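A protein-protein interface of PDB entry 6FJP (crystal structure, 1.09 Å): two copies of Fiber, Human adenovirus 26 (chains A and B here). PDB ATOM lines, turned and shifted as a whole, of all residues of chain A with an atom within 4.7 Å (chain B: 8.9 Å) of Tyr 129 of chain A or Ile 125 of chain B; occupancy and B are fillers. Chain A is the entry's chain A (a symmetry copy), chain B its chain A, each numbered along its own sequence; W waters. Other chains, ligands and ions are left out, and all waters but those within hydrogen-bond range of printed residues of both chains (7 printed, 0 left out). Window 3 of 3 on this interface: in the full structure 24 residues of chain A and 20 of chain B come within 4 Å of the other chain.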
ATOM      1  N   ASN A 127      -1.843  29.657   9.556  1.00  0.00           N
ATOM      2  CA  ASN A 127      -1.155  28.408   9.225  1.00  0.00           C
ATOM      3  C   ASN A 127      -0.635  28.447   7.812  1.00  0.00           C
ATOM      4  O   ASN A 127      -1.332  28.975   6.907  1.00  0.00           O
ATOM      5  CB  ASN A 127      -2.106  27.223   9.304  1.00  0.00           C
ATOM      6  CG  ASN A 127      -2.478  26.879  10.699  1.00  0.00           C
ATOM      7  OD1 ASN A 127      -1.617  26.661  11.537  1.00  0.00           O
ATOM      8  ND2 ASN A 127      -3.765  26.770  10.956  1.00  0.00           N
ATOM      9  N   VAL A 128       0.549  27.886   7.618  1.00  0.00           N
ATOM     10  CA  VAL A 128       1.099  27.465   6.334  1.00  0.00           C
ATOM     11  C   VAL A 128       1.287  25.951   6.421  1.00  0.00           C
ATOM     12  O   VAL A 128       0.981  25.355   7.471  1.00  0.00           O
ATOM     13  CB  VAL A 128       2.369  28.221   5.962  1.00  0.00           C
ATOM     14  CG1 VAL A 128       2.085  29.689   5.762  1.00  0.00           C
ATOM     15  CG2 VAL A 128       3.470  28.026   7.008  1.00  0.00           C
ATOM     16  N   TYR A 129       1.741  25.317   5.345  1.00  0.00           N
ATOM     17  CA  TYR A 129       1.702  23.863   5.297  1.00  0.00           C
ATOM     18  C   TYR A 129       3.049  23.315   4.848  1.00  0.00           C
ATOM     19  O   TYR A 129       3.593  23.689   3.797  1.00  0.00           O
ATOM     20  CB  TYR A 129       0.528  23.383   4.398  1.00  0.00           C
ATOM     21  CG  TYR A 129      -0.758  23.711   5.093  1.00  0.00           C
ATOM     22  CD1 TYR A 129      -1.323  24.979   5.024  1.00  0.00           C
ATOM     23  CD2 TYR A 129      -1.358  22.771   5.930  1.00  0.00           C
ATOM     24  CE1 TYR A 129      -2.414  25.305   5.791  1.00  0.00           C
ATOM     25  CE2 TYR A 129      -2.465  23.109   6.698  1.00  0.00           C
ATOM     26  CZ  TYR A 129      -2.968  24.395   6.634  1.00  0.00           C
ATOM     27  OH  TYR A 129      -4.081  24.765   7.409  1.00  0.00           O
ATOM     28  N   LEU A 130       3.594  22.422   5.677  1.00  0.00           N
ATOM     29  CA  LEU A 130       4.903  21.834   5.426  1.00  0.00           C
ATOM     30  C   LEU A 130       4.834  20.884   4.244  1.00  0.00           C
ATOM     31  O   LEU A 130       3.965  19.994   4.189  1.00  0.00           O
ATOM     32  CB  LEU A 130       5.395  21.089   6.660  1.00  0.00           C
ATOM     33  CG  LEU A 130       6.925  20.850   6.615  1.00  0.00           C
ATOM     34  CD1 LEU A 130       7.665  21.854   7.447  1.00  0.00           C
ATOM     35  CD2 LEU A 130       7.380  19.469   6.782  1.00  0.00           C
ATOM     36  N   GLY A 131       5.725  21.081   3.258  1.00  0.00           N
ATOM     37  CA  GLY A 131       5.698  20.271   2.076  1.00  0.00           C
ATOM     38  C   GLY A 131       4.485  20.486   1.207  1.00  0.00           C
ATOM     39  O   GLY A 131       4.212  19.696   0.317  1.00  0.00           O
ATOM     40  N   ALA A 132       3.731  21.551   1.472  1.00  0.00           N
ATOM     41  CA  ALA A 132       2.465  21.773   0.791  1.00  0.00           C
ATOM     42  C   ALA A 132       1.552  20.572   0.947  1.00  0.00           C
ATOM     43  O   ALA A 132       0.780  20.272   0.021  1.00  0.00           O
ATOM     44  CB  ALA A 132       2.643  22.173  -0.668  1.00  0.00           C
ATOM     45  N   LEU A 133       1.585  19.946   2.120  1.00  0.00           N
ATOM     46  CA  LEU A 133       0.699  18.822   2.418  1.00  0.00           C
ATOM     47  C   LEU A 133      -0.339  19.303   3.425  1.00  0.00           C
ATOM     48  O   LEU A 133      -0.021  19.890   4.473  1.00  0.00           O
ATOM     49  CB  LEU A 133       1.506  17.651   2.955  1.00  0.00           C
ATOM     50  CG  LEU A 133       2.578  17.152   1.988  1.00  0.00           C
ATOM     51  CD1 LEU A 133       3.354  15.990   2.611  1.00  0.00           C
ATOM     52  CD2 LEU A 133       2.011  16.753   0.668  1.00  0.00           C
ATOM     53  N   THR A 134      -1.620  19.053   3.099  1.00  0.00           N
ATOM     54  CA  THR A 134      -2.718  19.710   3.843  1.00  0.00           C
ATOM     55  C   THR A 134      -2.840  19.235   5.248  1.00  0.00           C
ATOM     56  O   THR A 134      -3.440  19.963   6.071  1.00  0.00           O
ATOM     57  CB  THR A 134      -4.055  19.513   3.094  1.00  0.00           C
ATOM     58  OG1 THR A 134      -4.316  18.121   3.061  1.00  0.00           O
ATOM     59  CG2 THR A 134      -4.017  20.077   1.688  1.00  0.00           C
ATOM     60  N   GLN A 136      -0.298  18.859   7.258  1.00  0.00           N
ATOM     61  CA  GLN A 136       0.933  19.270   7.950  1.00  0.00           C
ATOM     62  C   GLN A 136       0.980  20.766   8.221  1.00  0.00           C
ATOM     63  O   GLN A 136       1.835  21.497   7.742  1.00  0.00           O
ATOM     64  CB  GLN A 136       2.176  18.833   7.174  1.00  0.00           C
ATOM     65  CG  GLN A 136       2.211  17.346   6.963  1.00  0.00           C
ATOM     66  CD  GLN A 136       3.550  16.762   6.627  1.00  0.00           C
ATOM     67  OE1 GLN A 136       3.894  15.688   7.054  1.00  0.00           O
ATOM     68  NE2 GLN A 136       4.323  17.462   5.810  1.00  0.00           N
ATOM     69  N   PRO A 137       0.054  21.248   9.061  1.00  0.00           N
ATOM     70  CA  PRO A 137       0.074  22.681   9.399  1.00  0.00           C
ATOM     71  C   PRO A 137       1.321  23.066  10.192  1.00  0.00           C
ATOM     72  O   PRO A 137       1.869  22.302  11.020  1.00  0.00           O
ATOM     73  CB  PRO A 137      -1.134  22.806  10.304  1.00  0.00           C
ATOM     74  CG  PRO A 137      -1.322  21.469  10.922  1.00  0.00           C
ATOM     75  CD  PRO A 137      -0.957  20.507   9.816  1.00  0.00           C
ATOM     76  N   VAL A 138       1.736  24.291   9.940  1.00  0.00           N
ATOM     77  CA  VAL A 138       2.810  24.993  10.666  1.00  0.00           C
ATOM     78  C   VAL A 138       2.235  26.369  10.961  1.00  0.00           C
ATOM     79  O   VAL A 138       1.765  27.063  10.047  1.00  0.00           O
ATOM     80  CB  VAL A 138       4.059  25.084   9.791  1.00  0.00           C
ATOM     81  CG1 VAL A 138       5.107  25.989  10.444  1.00  0.00           C
ATOM     82  CG2 VAL A 138       4.632  23.728   9.511  1.00  0.00           C
ATOM     83  N   ASP A 172      10.029  22.989   4.402  1.00  0.00           N
ATOM     84  CA  ASP A 172       9.655  23.817   3.267  1.00  0.00           C
ATOM     85  C   ASP A 172       8.188  24.122   3.493  1.00  0.00           C
ATOM     86  O   ASP A 172       7.448  23.206   3.945  1.00  0.00           O
ATOM     87  CB  ASP A 172       9.857  23.097   1.956  1.00  0.00           C
ATOM     88  CG  ASP A 172       9.774  24.040   0.740  1.00  0.00           C
ATOM     89  OD1 ASP A 172       9.729  25.256   0.937  1.00  0.00           O
ATOM     90  OD2 ASP A 172       9.808  23.540  -0.403  1.00  0.00           O
ATOM     91  N   VAL A 173       7.742  25.333   3.277  1.00  0.00           N
ATOM     92  CA  VAL A 173       6.330  25.703   3.536  1.00  0.00           C
ATOM     93  C   VAL A 173       5.724  26.433   2.346  1.00  0.00           C
ATOM     94  O   VAL A 173       6.424  27.051   1.514  1.00  0.00           O
ATOM     95  CB  VAL A 173       6.192  26.533   4.798  1.00  0.00           C
ATOM     96  CG1 VAL A 173       6.469  25.732   6.052  1.00  0.00           C
ATOM     97  CG2 VAL A 173       7.055  27.801   4.764  1.00  0.00           C
ATOM     98  N   THR A 174       4.408  26.333   2.260  1.00  0.00           N
ATOM     99  CA  THR A 174       3.634  27.107   1.330  1.00  0.00           C
ATOM    100  C   THR A 174       3.827  28.603   1.525  1.00  0.00           C
ATOM    101  O   THR A 174       4.290  29.058   2.580  1.00  0.00           O
ATOM    102  CB  THR A 174       2.152  26.717   1.439  1.00  0.00           C
ATOM    103  OG1 THR A 174       1.702  26.844   2.796  1.00  0.00           O
ATOM    104  CG2 THR A 174       1.914  25.313   0.967  1.00  0.00           C
ATOM    105  N   LYS B 117      13.568  19.667  -5.879  1.00  0.00           N
ATOM    106  CA  LYS B 117      12.419  19.154  -5.135  1.00  0.00           C
ATOM    107  C   LYS B 117      11.134  19.718  -5.734  1.00  0.00           C
ATOM    108  O   LYS B 117      11.185  20.564  -6.628  1.00  0.00           O
ATOM    109  CB  LYS B 117      12.552  19.422  -3.594  1.00  0.00           C
ATOM    110  CG  LYS B 117      12.019  20.725  -3.055  1.00  0.00           C
ATOM    111  CD  LYS B 117      12.391  21.103  -1.610  1.00  0.00           C
ATOM    112  CE  LYS B 117      11.565  20.483  -0.496  1.00  0.00           C
ATOM    113  NZ  LYS B 117      10.135  20.815  -0.604  1.00  0.00           N
ATOM    114  N   TYR B 119       8.934  22.332  -4.952  1.00  0.00           N
ATOM    115  CA  TYR B 119       9.039  23.542  -4.017  1.00  0.00           C
ATOM    116  C   TYR B 119       7.733  23.979  -3.451  1.00  0.00           C
ATOM    117  O   TYR B 119       6.819  24.297  -4.208  1.00  0.00           O
ATOM    118  CB  TYR B 119       9.677  24.709  -4.741  1.00  0.00           C
ATOM    119  CG  TYR B 119      11.119  24.465  -5.096  1.00  0.00           C
ATOM    120  CD1 TYR B 119      12.096  24.518  -4.120  1.00  0.00           C
ATOM    121  CD2 TYR B 119      11.543  24.137  -6.377  1.00  0.00           C
ATOM    122  CE1 TYR B 119      13.421  24.310  -4.373  1.00  0.00           C
ATOM    123  CE2 TYR B 119      12.897  23.907  -6.653  1.00  0.00           C
ATOM    124  CZ  TYR B 119      13.832  24.019  -5.632  1.00  0.00           C
ATOM    125  OH  TYR B 119      15.178  23.810  -5.816  1.00  0.00           O
ATOM    126  N   SER B 120       7.603  23.962  -2.137  1.00  0.00           N
ATOM    127  CA  SER B 120       6.328  24.224  -1.535  1.00  0.00           C
ATOM    128  C   SER B 120       5.822  25.651  -1.753  1.00  0.00           C
ATOM    129  O   SER B 120       4.645  25.874  -1.676  1.00  0.00           O
ATOM    130  CB  SER B 120       6.361  23.891  -0.039  1.00  0.00           C
ATOM    131  OG  SER B 120       6.769  22.573   0.177  1.00  0.00           O
ATOM    132  N   ARG B 121       6.757  26.580  -2.013  1.00  0.00           N
ATOM    133  CA  ARG B 121       6.330  27.975  -2.198  1.00  0.00           C
ATOM    134  C   ARG B 121       5.481  28.158  -3.459  1.00  0.00           C
ATOM    135  O   ARG B 121       4.808  29.188  -3.608  1.00  0.00           O
ATOM    136  CB  ARG B 121       7.520  28.913  -2.227  1.00  0.00           C
ATOM    137  CG  ARG B 121       8.350  28.814  -3.504  1.00  0.00           C
ATOM    138  CD  ARG B 121       9.590  29.668  -3.414  1.00  0.00           C
ATOM    139  NE  ARG B 121      10.316  29.607  -4.686  1.00  0.00           N
ATOM    140  CZ  ARG B 121      11.549  30.004  -4.901  1.00  0.00           C
ATOM    141  NH1 ARG B 121      12.276  30.641  -3.971  1.00  0.00           N
ATOM    142  NH2 ARG B 121      12.075  29.771  -6.082  1.00  0.00           N
ATOM    143  N   THR B 122       5.435  27.160  -4.343  1.00  0.00           N
ATOM    144  CA  THR B 122       4.566  27.161  -5.512  1.00  0.00           C
ATOM    145  C   THR B 122       3.088  27.023  -5.158  1.00  0.00           C
ATOM    146  O   THR B 122       2.261  27.133  -6.091  1.00  0.00           O
ATOM    147  CB  THR B 122       4.957  26.084  -6.534  1.00  0.00           C
ATOM    148  OG1 THR B 122       4.740  24.803  -5.972  1.00  0.00           O
ATOM    149  CG2 THR B 122       6.394  26.222  -7.021  1.00  0.00           C
ATOM    150  N   LYS B 123       2.768  26.730  -3.912  1.00  0.00           N
ATOM    151  CA  LYS B 123       1.398  26.607  -3.482  1.00  0.00           C
ATOM    152  C   LYS B 123       1.085  27.527  -2.335  1.00  0.00           C
ATOM    153  O   LYS B 123       1.950  27.911  -1.532  1.00  0.00           O
ATOM    154  CB  LYS B 123       1.099  25.178  -3.065  1.00  0.00           C
ATOM    155  CG  LYS B 123       1.023  24.266  -4.267  1.00  0.00           C
ATOM    156  CD  LYS B 123       0.881  22.830  -3.968  1.00  0.00           C
ATOM    157  CE  LYS B 123       0.627  21.992  -5.187  1.00  0.00           C
ATOM    158  NZ  LYS B 123       0.417  20.554  -4.825  1.00  0.00           N
ATOM    159  N   ILE B 124      -0.207  27.882  -2.262  1.00  0.00           N
ATOM    160  CA  ILE B 124      -0.835  28.517  -1.091  1.00  0.00           C
ATOM    161  C   ILE B 124      -1.894  27.558  -0.625  1.00  0.00           C
ATOM    162  O   ILE B 124      -2.696  27.083  -1.469  1.00  0.00           O
ATOM    163  CB  ILE B 124      -1.509  29.851  -1.473  1.00  0.00           C
ATOM    164  CG1 ILE B 124      -0.491  30.831  -2.048  1.00  0.00           C
ATOM    165  CG2 ILE B 124      -2.253  30.413  -0.284  1.00  0.00           C
ATOM    166  CD1 ILE B 124      -1.193  31.919  -2.884  1.00  0.00           C
ATOM    167  N   ILE B 125      -1.944  27.232   0.669  1.00  0.00           N
ATOM    168  CA  ILE B 125      -2.967  26.360   1.178  1.00  0.00           C
ATOM    169  C   ILE B 125      -3.623  27.033   2.373  1.00  0.00           C
ATOM    170  O   ILE B 125      -2.910  27.501   3.290  1.00  0.00           O
ATOM    171  CB  ILE B 125      -2.385  24.990   1.589  1.00  0.00           C
ATOM    172  CG1 ILE B 125      -1.916  24.227   0.357  1.00  0.00           C
ATOM    173  CG2 ILE B 125      -3.423  24.146   2.313  1.00  0.00           C
ATOM    174  CD1 ILE B 125      -1.177  22.944   0.627  1.00  0.00           C
ATOM    175  N   SER B 126      -4.938  27.094   2.376  1.00  0.00           N
ATOM    176  CA  SER B 126      -5.678  27.652   3.523  1.00  0.00           C
ATOM    177  C   SER B 126      -7.047  27.066   3.545  1.00  0.00           C
ATOM    178  O   SER B 126      -7.319  26.076   2.819  1.00  0.00           O
ATOM    179  CB  SER B 126      -5.680  29.184   3.430  1.00  0.00           C
ATOM    180  OG  SER B 126      -6.128  29.757   4.654  1.00  0.00           O
ATOM    181  N   ASN B 127      -7.939  27.581   4.390  1.00  0.00           N
ATOM    182  CA  ASN B 127      -9.338  27.154   4.409  1.00  0.00           C
ATOM    183  C   ASN B 127     -10.240  28.270   3.950  1.00  0.00           C
ATOM    184  O   ASN B 127      -9.996  29.452   4.305  1.00  0.00           O
ATOM    185  CB  ASN B 127      -9.780  26.793   5.820  1.00  0.00           C
ATOM    186  CG  ASN B 127      -9.180  25.523   6.301  1.00  0.00           C
ATOM    187  OD1 ASN B 127      -9.296  24.496   5.651  1.00  0.00           O
ATOM    188  ND2 ASN B 127      -8.579  25.562   7.472  1.00  0.00           N
ATOM    189  N   VAL B 128     -11.269  27.908   3.198  1.00  0.00           N
ATOM    190  CA  VAL B 128     -12.463  28.703   2.937  1.00  0.00           C
ATOM    191  C   VAL B 128     -13.638  27.918   3.519  1.00  0.00           C
ATOM    192  O   VAL B 128     -13.430  26.820   4.069  1.00  0.00           O
ATOM    193  CB  VAL B 128     -12.628  29.052   1.464  1.00  0.00           C
ATOM    194  CG1 VAL B 128     -11.503  29.938   0.989  1.00  0.00           C
ATOM    195  CG2 VAL B 128     -12.725  27.797   0.592  1.00  0.00           C
ATOM    196  N   TYR B 129     -14.848  28.461   3.445  1.00  0.00           N
ATOM    197  CA  TYR B 129     -15.948  27.873   4.196  1.00  0.00           C
ATOM    198  C   TYR B 129     -17.164  27.699   3.298  1.00  0.00           C
ATOM    199  O   TYR B 129     -17.643  28.642   2.649  1.00  0.00           O
ATOM    200  CB  TYR B 129     -16.253  28.723   5.462  1.00  0.00           C
ATOM    201  CG  TYR B 129     -15.106  28.574   6.413  1.00  0.00           C
ATOM    202  CD1 TYR B 129     -13.945  29.325   6.282  1.00  0.00           C
ATOM    203  CD2 TYR B 129     -15.135  27.579   7.392  1.00  0.00           C
ATOM    204  CE1 TYR B 129     -12.846  29.066   7.064  1.00  0.00           C
ATOM    205  CE2 TYR B 129     -14.020  27.328   8.182  1.00  0.00           C
ATOM    206  CZ  TYR B 129     -12.870  28.069   7.986  1.00  0.00           C
ATOM    207  OH  TYR B 129     -11.725  27.828   8.766  1.00  0.00           O
ATOM    208  N   VAL B 138     -13.318  24.034   3.914  1.00  0.00           N
ATOM    209  CA  VAL B 138     -12.889  23.456   2.628  1.00  0.00           C
ATOM    210  C   VAL B 138     -11.461  23.943   2.447  1.00  0.00           C
ATOM    211  O   VAL B 138     -11.194  25.151   2.523  1.00  0.00           O
ATOM    212  CB  VAL B 138     -13.797  23.953   1.504  1.00  0.00           C
ATOM    213  CG1 VAL B 138     -13.241  23.535   0.140  1.00  0.00           C
ATOM    214  CG2 VAL B 138     -15.202  23.463   1.675  1.00  0.00           C
ATOM    215  N   ILE B 139     -10.537  23.030   2.161  1.00  0.00           N
ATOM    216  CA  ILE B 139      -9.147  23.444   1.917  1.00  0.00           C
ATOM    217  C   ILE B 139      -9.074  24.017   0.519  1.00  0.00           C
ATOM    218  O   ILE B 139      -9.467  23.321  -0.454  1.00  0.00           O
ATOM    219  CB  ILE B 139      -8.202  22.259   2.053  1.00  0.00           C
ATOM    220  CG1 ILE B 139      -8.343  21.605   3.441  1.00  0.00           C
ATOM    221  CG2 ILE B 139      -6.807  22.696   1.762  1.00  0.00           C
ATOM    222  CD1 ILE B 139      -7.881  20.143   3.445  1.00  0.00           C
ATOM    223  N   ILE B 140      -8.526  25.200   0.367  1.00  0.00           N
ATOM    224  CA  ILE B 140      -8.173  25.759  -0.914  1.00  0.00           C
ATOM    225  C   ILE B 140      -6.673  25.616  -1.113  1.00  0.00           C
ATOM    226  O   ILE B 140      -5.881  25.998  -0.238  1.00  0.00           O
ATOM    227  CB  ILE B 140      -8.637  27.214  -1.079  1.00  0.00           C
ATOM    228  CG1 ILE B 140      -8.388  27.686  -2.496  1.00  0.00           C
ATOM    229  CG2 ILE B 140      -8.042  28.181  -0.060  1.00  0.00           C
ATOM    230  CD1 ILE B 140      -8.933  29.065  -2.841  1.00  0.00           C
ATOM    231  N   THR B 141      -6.289  25.069  -2.278  1.00  0.00           N
ATOM    232  CA  THR B 141      -4.897  24.981  -2.679  1.00  0.00           C
ATOM    233  C   THR B 141      -4.766  25.758  -3.956  1.00  0.00           C
ATOM    234  O   THR B 141      -5.390  25.363  -4.984  1.00  0.00           O
ATOM    235  CB  THR B 141      -4.427  23.537  -2.903  1.00  0.00           C
ATOM    236  OG1 THR B 141      -4.576  22.789  -1.709  1.00  0.00           O
ATOM    237  CG2 THR B 141      -2.960  23.524  -3.265  1.00  0.00           C
ATOM    238  N   ILE B 142      -3.969  26.801  -3.973  1.00  0.00           N
ATOM    239  CA  ILE B 142      -3.655  27.548  -5.182  1.00  0.00           C
ATOM    240  C   ILE B 142      -2.263  27.178  -5.601  1.00  0.00           C
ATOM    241  O   ILE B 142      -1.354  27.261  -4.786  1.00  0.00           O
ATOM    242  CB  ILE B 142      -3.794  29.062  -4.982  1.00  0.00           C
ATOM    243  CG1 ILE B 142      -5.128  29.390  -4.295  1.00  0.00           C
ATOM    244  CG2 ILE B 142      -3.638  29.770  -6.315  1.00  0.00           C
ATOM    245  CD1 ILE B 142      -5.369  30.864  -4.077  1.00  0.00           C
ATOM    246  N   ALA B 143      -2.080  26.776  -6.856  1.00  0.00           N
ATOM    247  CA  ALA B 143      -0.783  26.345  -7.324  1.00  0.00           C
ATOM    248  C   ALA B 143      -0.398  27.159  -8.541  1.00  0.00           C
ATOM    249  O   ALA B 143      -1.210  27.356  -9.467  1.00  0.00           O
ATOM    250  CB  ALA B 143      -0.764  24.863  -7.670  1.00  0.00           C
ATOM    251  N   PHE B 144       0.886  27.539  -8.619  1.00  0.00           N
ATOM    252  CA  PHE B 144       1.407  28.384  -9.674  1.00  0.00           C
ATOM    253  C   PHE B 144       2.376  27.621 -10.553  1.00  0.00           C
ATOM    254  O   PHE B 144       3.388  27.078 -10.048  1.00  0.00           O
ATOM    255  CB  PHE B 144       2.115  29.597  -9.065  1.00  0.00           C
ATOM    256  CG  PHE B 144       1.187  30.403  -8.216  1.00  0.00           C
ATOM    257  CD1 PHE B 144       0.187  31.160  -8.790  1.00  0.00           C
ATOM    258  CD2 PHE B 144       1.268  30.399  -6.839  1.00  0.00           C
ATOM    259  CE1 PHE B 144      -0.742  31.851  -8.020  1.00  0.00           C
ATOM    260  CE2 PHE B 144       0.343  31.098  -6.041  1.00  0.00           C
ATOM    261  CZ  PHE B 144      -0.673  31.801  -6.678  1.00  0.00           C
ATOM    262  N   THR B 159      -7.678  24.307  -6.249  1.00  0.00           N
ATOM    263  CA  THR B 159      -8.244  23.027  -5.865  1.00  0.00           C
ATOM    264  C   THR B 159      -8.980  23.233  -4.555  1.00  0.00           C
ATOM    265  O   THR B 159      -8.497  23.948  -3.648  1.00  0.00           O
ATOM    266  CB  THR B 159      -7.168  21.978  -5.693  1.00  0.00           C
ATOM    267  OG1 THR B 159      -6.471  21.821  -6.949  1.00  0.00           O
ATOM    268  CG2 THR B 159      -7.741  20.602  -5.351  1.00  0.00           C
ATOM    269  N   THR B 161     -10.679  20.923  -1.538  1.00  0.00           N
ATOM    270  CA  THR B 161     -10.623  19.574  -1.028  1.00  0.00           C
ATOM    271  C   THR B 161     -11.222  19.532   0.364  1.00  0.00           C
ATOM    272  O   THR B 161     -10.942  20.451   1.180  1.00  0.00           O
ATOM    273  CB  THR B 161      -9.154  19.097  -0.892  1.00  0.00           C
ATOM    274  OG1 THR B 161      -8.432  19.336  -2.116  1.00  0.00           O
ATOM    275  CG2 THR B 161      -9.044  17.634  -0.563  1.00  0.00           C
ATOM    276  N   PHE B 176     -11.538  34.319  -1.020  1.00  0.00           N
ATOM    277  CA  PHE B 176     -10.174  34.149  -0.545  1.00  0.00           C
ATOM    278  C   PHE B 176      -9.235  35.116  -1.250  1.00  0.00           C
ATOM    279  O   PHE B 176      -9.215  35.160  -2.488  1.00  0.00           O
ATOM    280  CB  PHE B 176      -9.731  32.713  -0.785  1.00  0.00           C
ATOM    281  CG  PHE B 176      -8.399  32.385  -0.164  1.00  0.00           C
ATOM    282  CD1 PHE B 176      -8.242  32.303   1.194  1.00  0.00           C
ATOM    283  CD2 PHE B 176      -7.275  32.211  -0.944  1.00  0.00           C
ATOM    284  CE1 PHE B 176      -7.022  32.027   1.764  1.00  0.00           C
ATOM    285  CE2 PHE B 176      -6.023  31.940  -0.371  1.00  0.00           C
ATOM    286  CZ  PHE B 176      -5.920  31.866   0.963  1.00  0.00           C
ATOM    287  N   PHE B 178      -5.270  36.458  -1.909  1.00  0.00           N
ATOM    288  CA  PHE B 178      -3.929  35.885  -2.008  1.00  0.00           C
ATOM    289  C   PHE B 178      -3.062  36.788  -2.843  1.00  0.00           C
ATOM    290  O   PHE B 178      -3.561  37.780  -3.444  1.00  0.00           O
ATOM    291  CB  PHE B 178      -3.991  34.471  -2.601  1.00  0.00           C
ATOM    292  CG  PHE B 178      -4.512  34.415  -4.008  1.00  0.00           C
ATOM    293  CD1 PHE B 178      -5.888  34.396  -4.252  1.00  0.00           C
ATOM    294  CD2 PHE B 178      -3.662  34.299  -5.093  1.00  0.00           C
ATOM    295  CE1 PHE B 178      -6.377  34.326  -5.548  1.00  0.00           C
ATOM    296  CE2 PHE B 178      -4.161  34.223  -6.389  1.00  0.00           C
ATOM    297  CZ  PHE B 178      -5.516  34.228  -6.626  1.00  0.00           C
HETATM  298  O   HOH W   1      -5.492  27.041   7.250  1.00  0.00           O
HETATM  299  O   HOH W   2      -4.200  29.217   6.767  1.00  0.00           O
HETATM  300  O   HOH W   3      -6.086  24.543   5.277  1.00  0.00           O
HETATM  301  O   HOH W   4       6.259  20.747  -1.819  1.00  0.00           O
HETATM  302  O   HOH W   5      -1.697  29.691   4.316  1.00  0.00           O
HETATM  303  O   HOH W   6       0.025  28.868   2.358  1.00  0.00           O
HETATM  304  O   HOH W   7       9.658  26.203  -1.862  1.00  0.00           O
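Printed residues of chain B that touch a printed residue of chain A: Lys 117, Tyr 119, Ser 120, Arg 121, Lys 123, Ile 125 and Ile 139. Hydrophobic or aromatic side chains of chain B that line the printed part of chain A: Ile 125 and Ile 139. Of the 14 printed residues of chain A, 7 touch a printed residue of chain B. Among the printed residues, Asp or Glu carboxylates within 4 Å of a Lys or Arg side-chain nitrogen of the other chain: Asp 172 of chain A with Lys 117 of chain B.
Printed residues of chain B within 4 Å of Tyr 129 of chain A: Ile 125 (3.4 Å). Ile 125 of chain B touches three residues of chain A. Of the printed residues of chain B, Thr 174 of chain A touches Ser 120 (3.4 Å), Lys 123 (3.2 Å) and Ile 125 (3.9 Å). Printed residues of chain B within 4 Å of Asp 172 of chain A: Lys 117, Tyr 119 and Ser 120. Val 138 of chain B touches none of the printed residues of chain A.
CE1 of Tyr 129 of chain A touches O of Ile 125 of chain B, at 3.4 Å. Ala 132 of chain A touches Lys 123 of chain B. Ala 132 of chain A touches Ile 125 of chain B. Ile 139 of chain B touches Thr 134 of chain A. OD2 of Asp 172 of chain A touches CA of Tyr 119 of chain B (3.7 Å). O of Val 173 of chain A touches CB of Ser 120 of chain B (3.5 Å). Val 173 of chain A touches Arg 121 of chain B. Thr 174 of chain A touches Ser 120 of chain B. Thr 174 of chain A touches Lys 123 of chain B. Thr 174 of chain A touches Ile 125 of chain B (CG2 to CD1, 3.9 Å).
The backbone carbonyl oxygen (O) of Tyr 119 of chain B lies within hydrogen-bond range of the side-chain hydroxyl (OG1) of Thr 122 of chain B (2.8 Å). N of Gly 131 of chain A is in hydrogen-bond range of O of Asp 172 of chain A (2.8 Å). The backbone NH (N) of Tyr 129 of chain A lies within hydrogen-bond range of the side-chain hydroxyl (OG1) of Thr 174 of chain A, 3.0 Å away. N of Ile 139 of chain B lies within hydrogen-bond range of O of Thr 161 of chain B (2.8 Å).
Water W6 lies within hydrogen-bond range of the side-chain hydroxyl of Thr 174 of chain A and the backbone NH of Ile 125 of chain B. Water W1 lies within hydrogen-bond range of OH of Tyr 129 of chain A (2.7 Å) and ND2 of Asn 127 of chain B (3.4 Å). Water W4 lies within hydrogen-bond range of the side-chain hydroxyl of Ser 120 of chain B (2.8 Å) and the backbone carbonyl oxygen of Gly 131 of chain A (3.1 Å). Water W2 bridges the backbone carbonyl oxygen of Asn 127 of chain A (2.9 Å) and the side-chain hydroxyl of Ser 126 of chain B (2.9 Å). Water W3 lies within hydrogen-bond range of the side-chain hydroxyl of Tyr 129 of chain A (2.9 Å), the backbone carbonyl oxygen of Ser 126 of chain B (3.1 Å) and the side-chain amide oxygen of Asn 127 of chain B (3.2 Å).
4 positions are printed for both chains. Of the 14 pairs that touch across the chains among the printed residues, none has its exchanged pair printed and touching as well.
N of Ser 120 of chain B is in hydrogen-bond range of OD2 of Asp 172 of chain A, 2.8 Å away. The side-chain hydroxyl (OG) of Ser 120 of chain B is in hydrogen-bond range of the backbone NH (N) of Ala 132 of chain A (3.5 Å). The side-chain carboxylate (OD2) of Asp 172 of chain A is in salt-bridge range of the side-chain amino group (NZ) of Lys 117 of chain B (2.8 Å).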
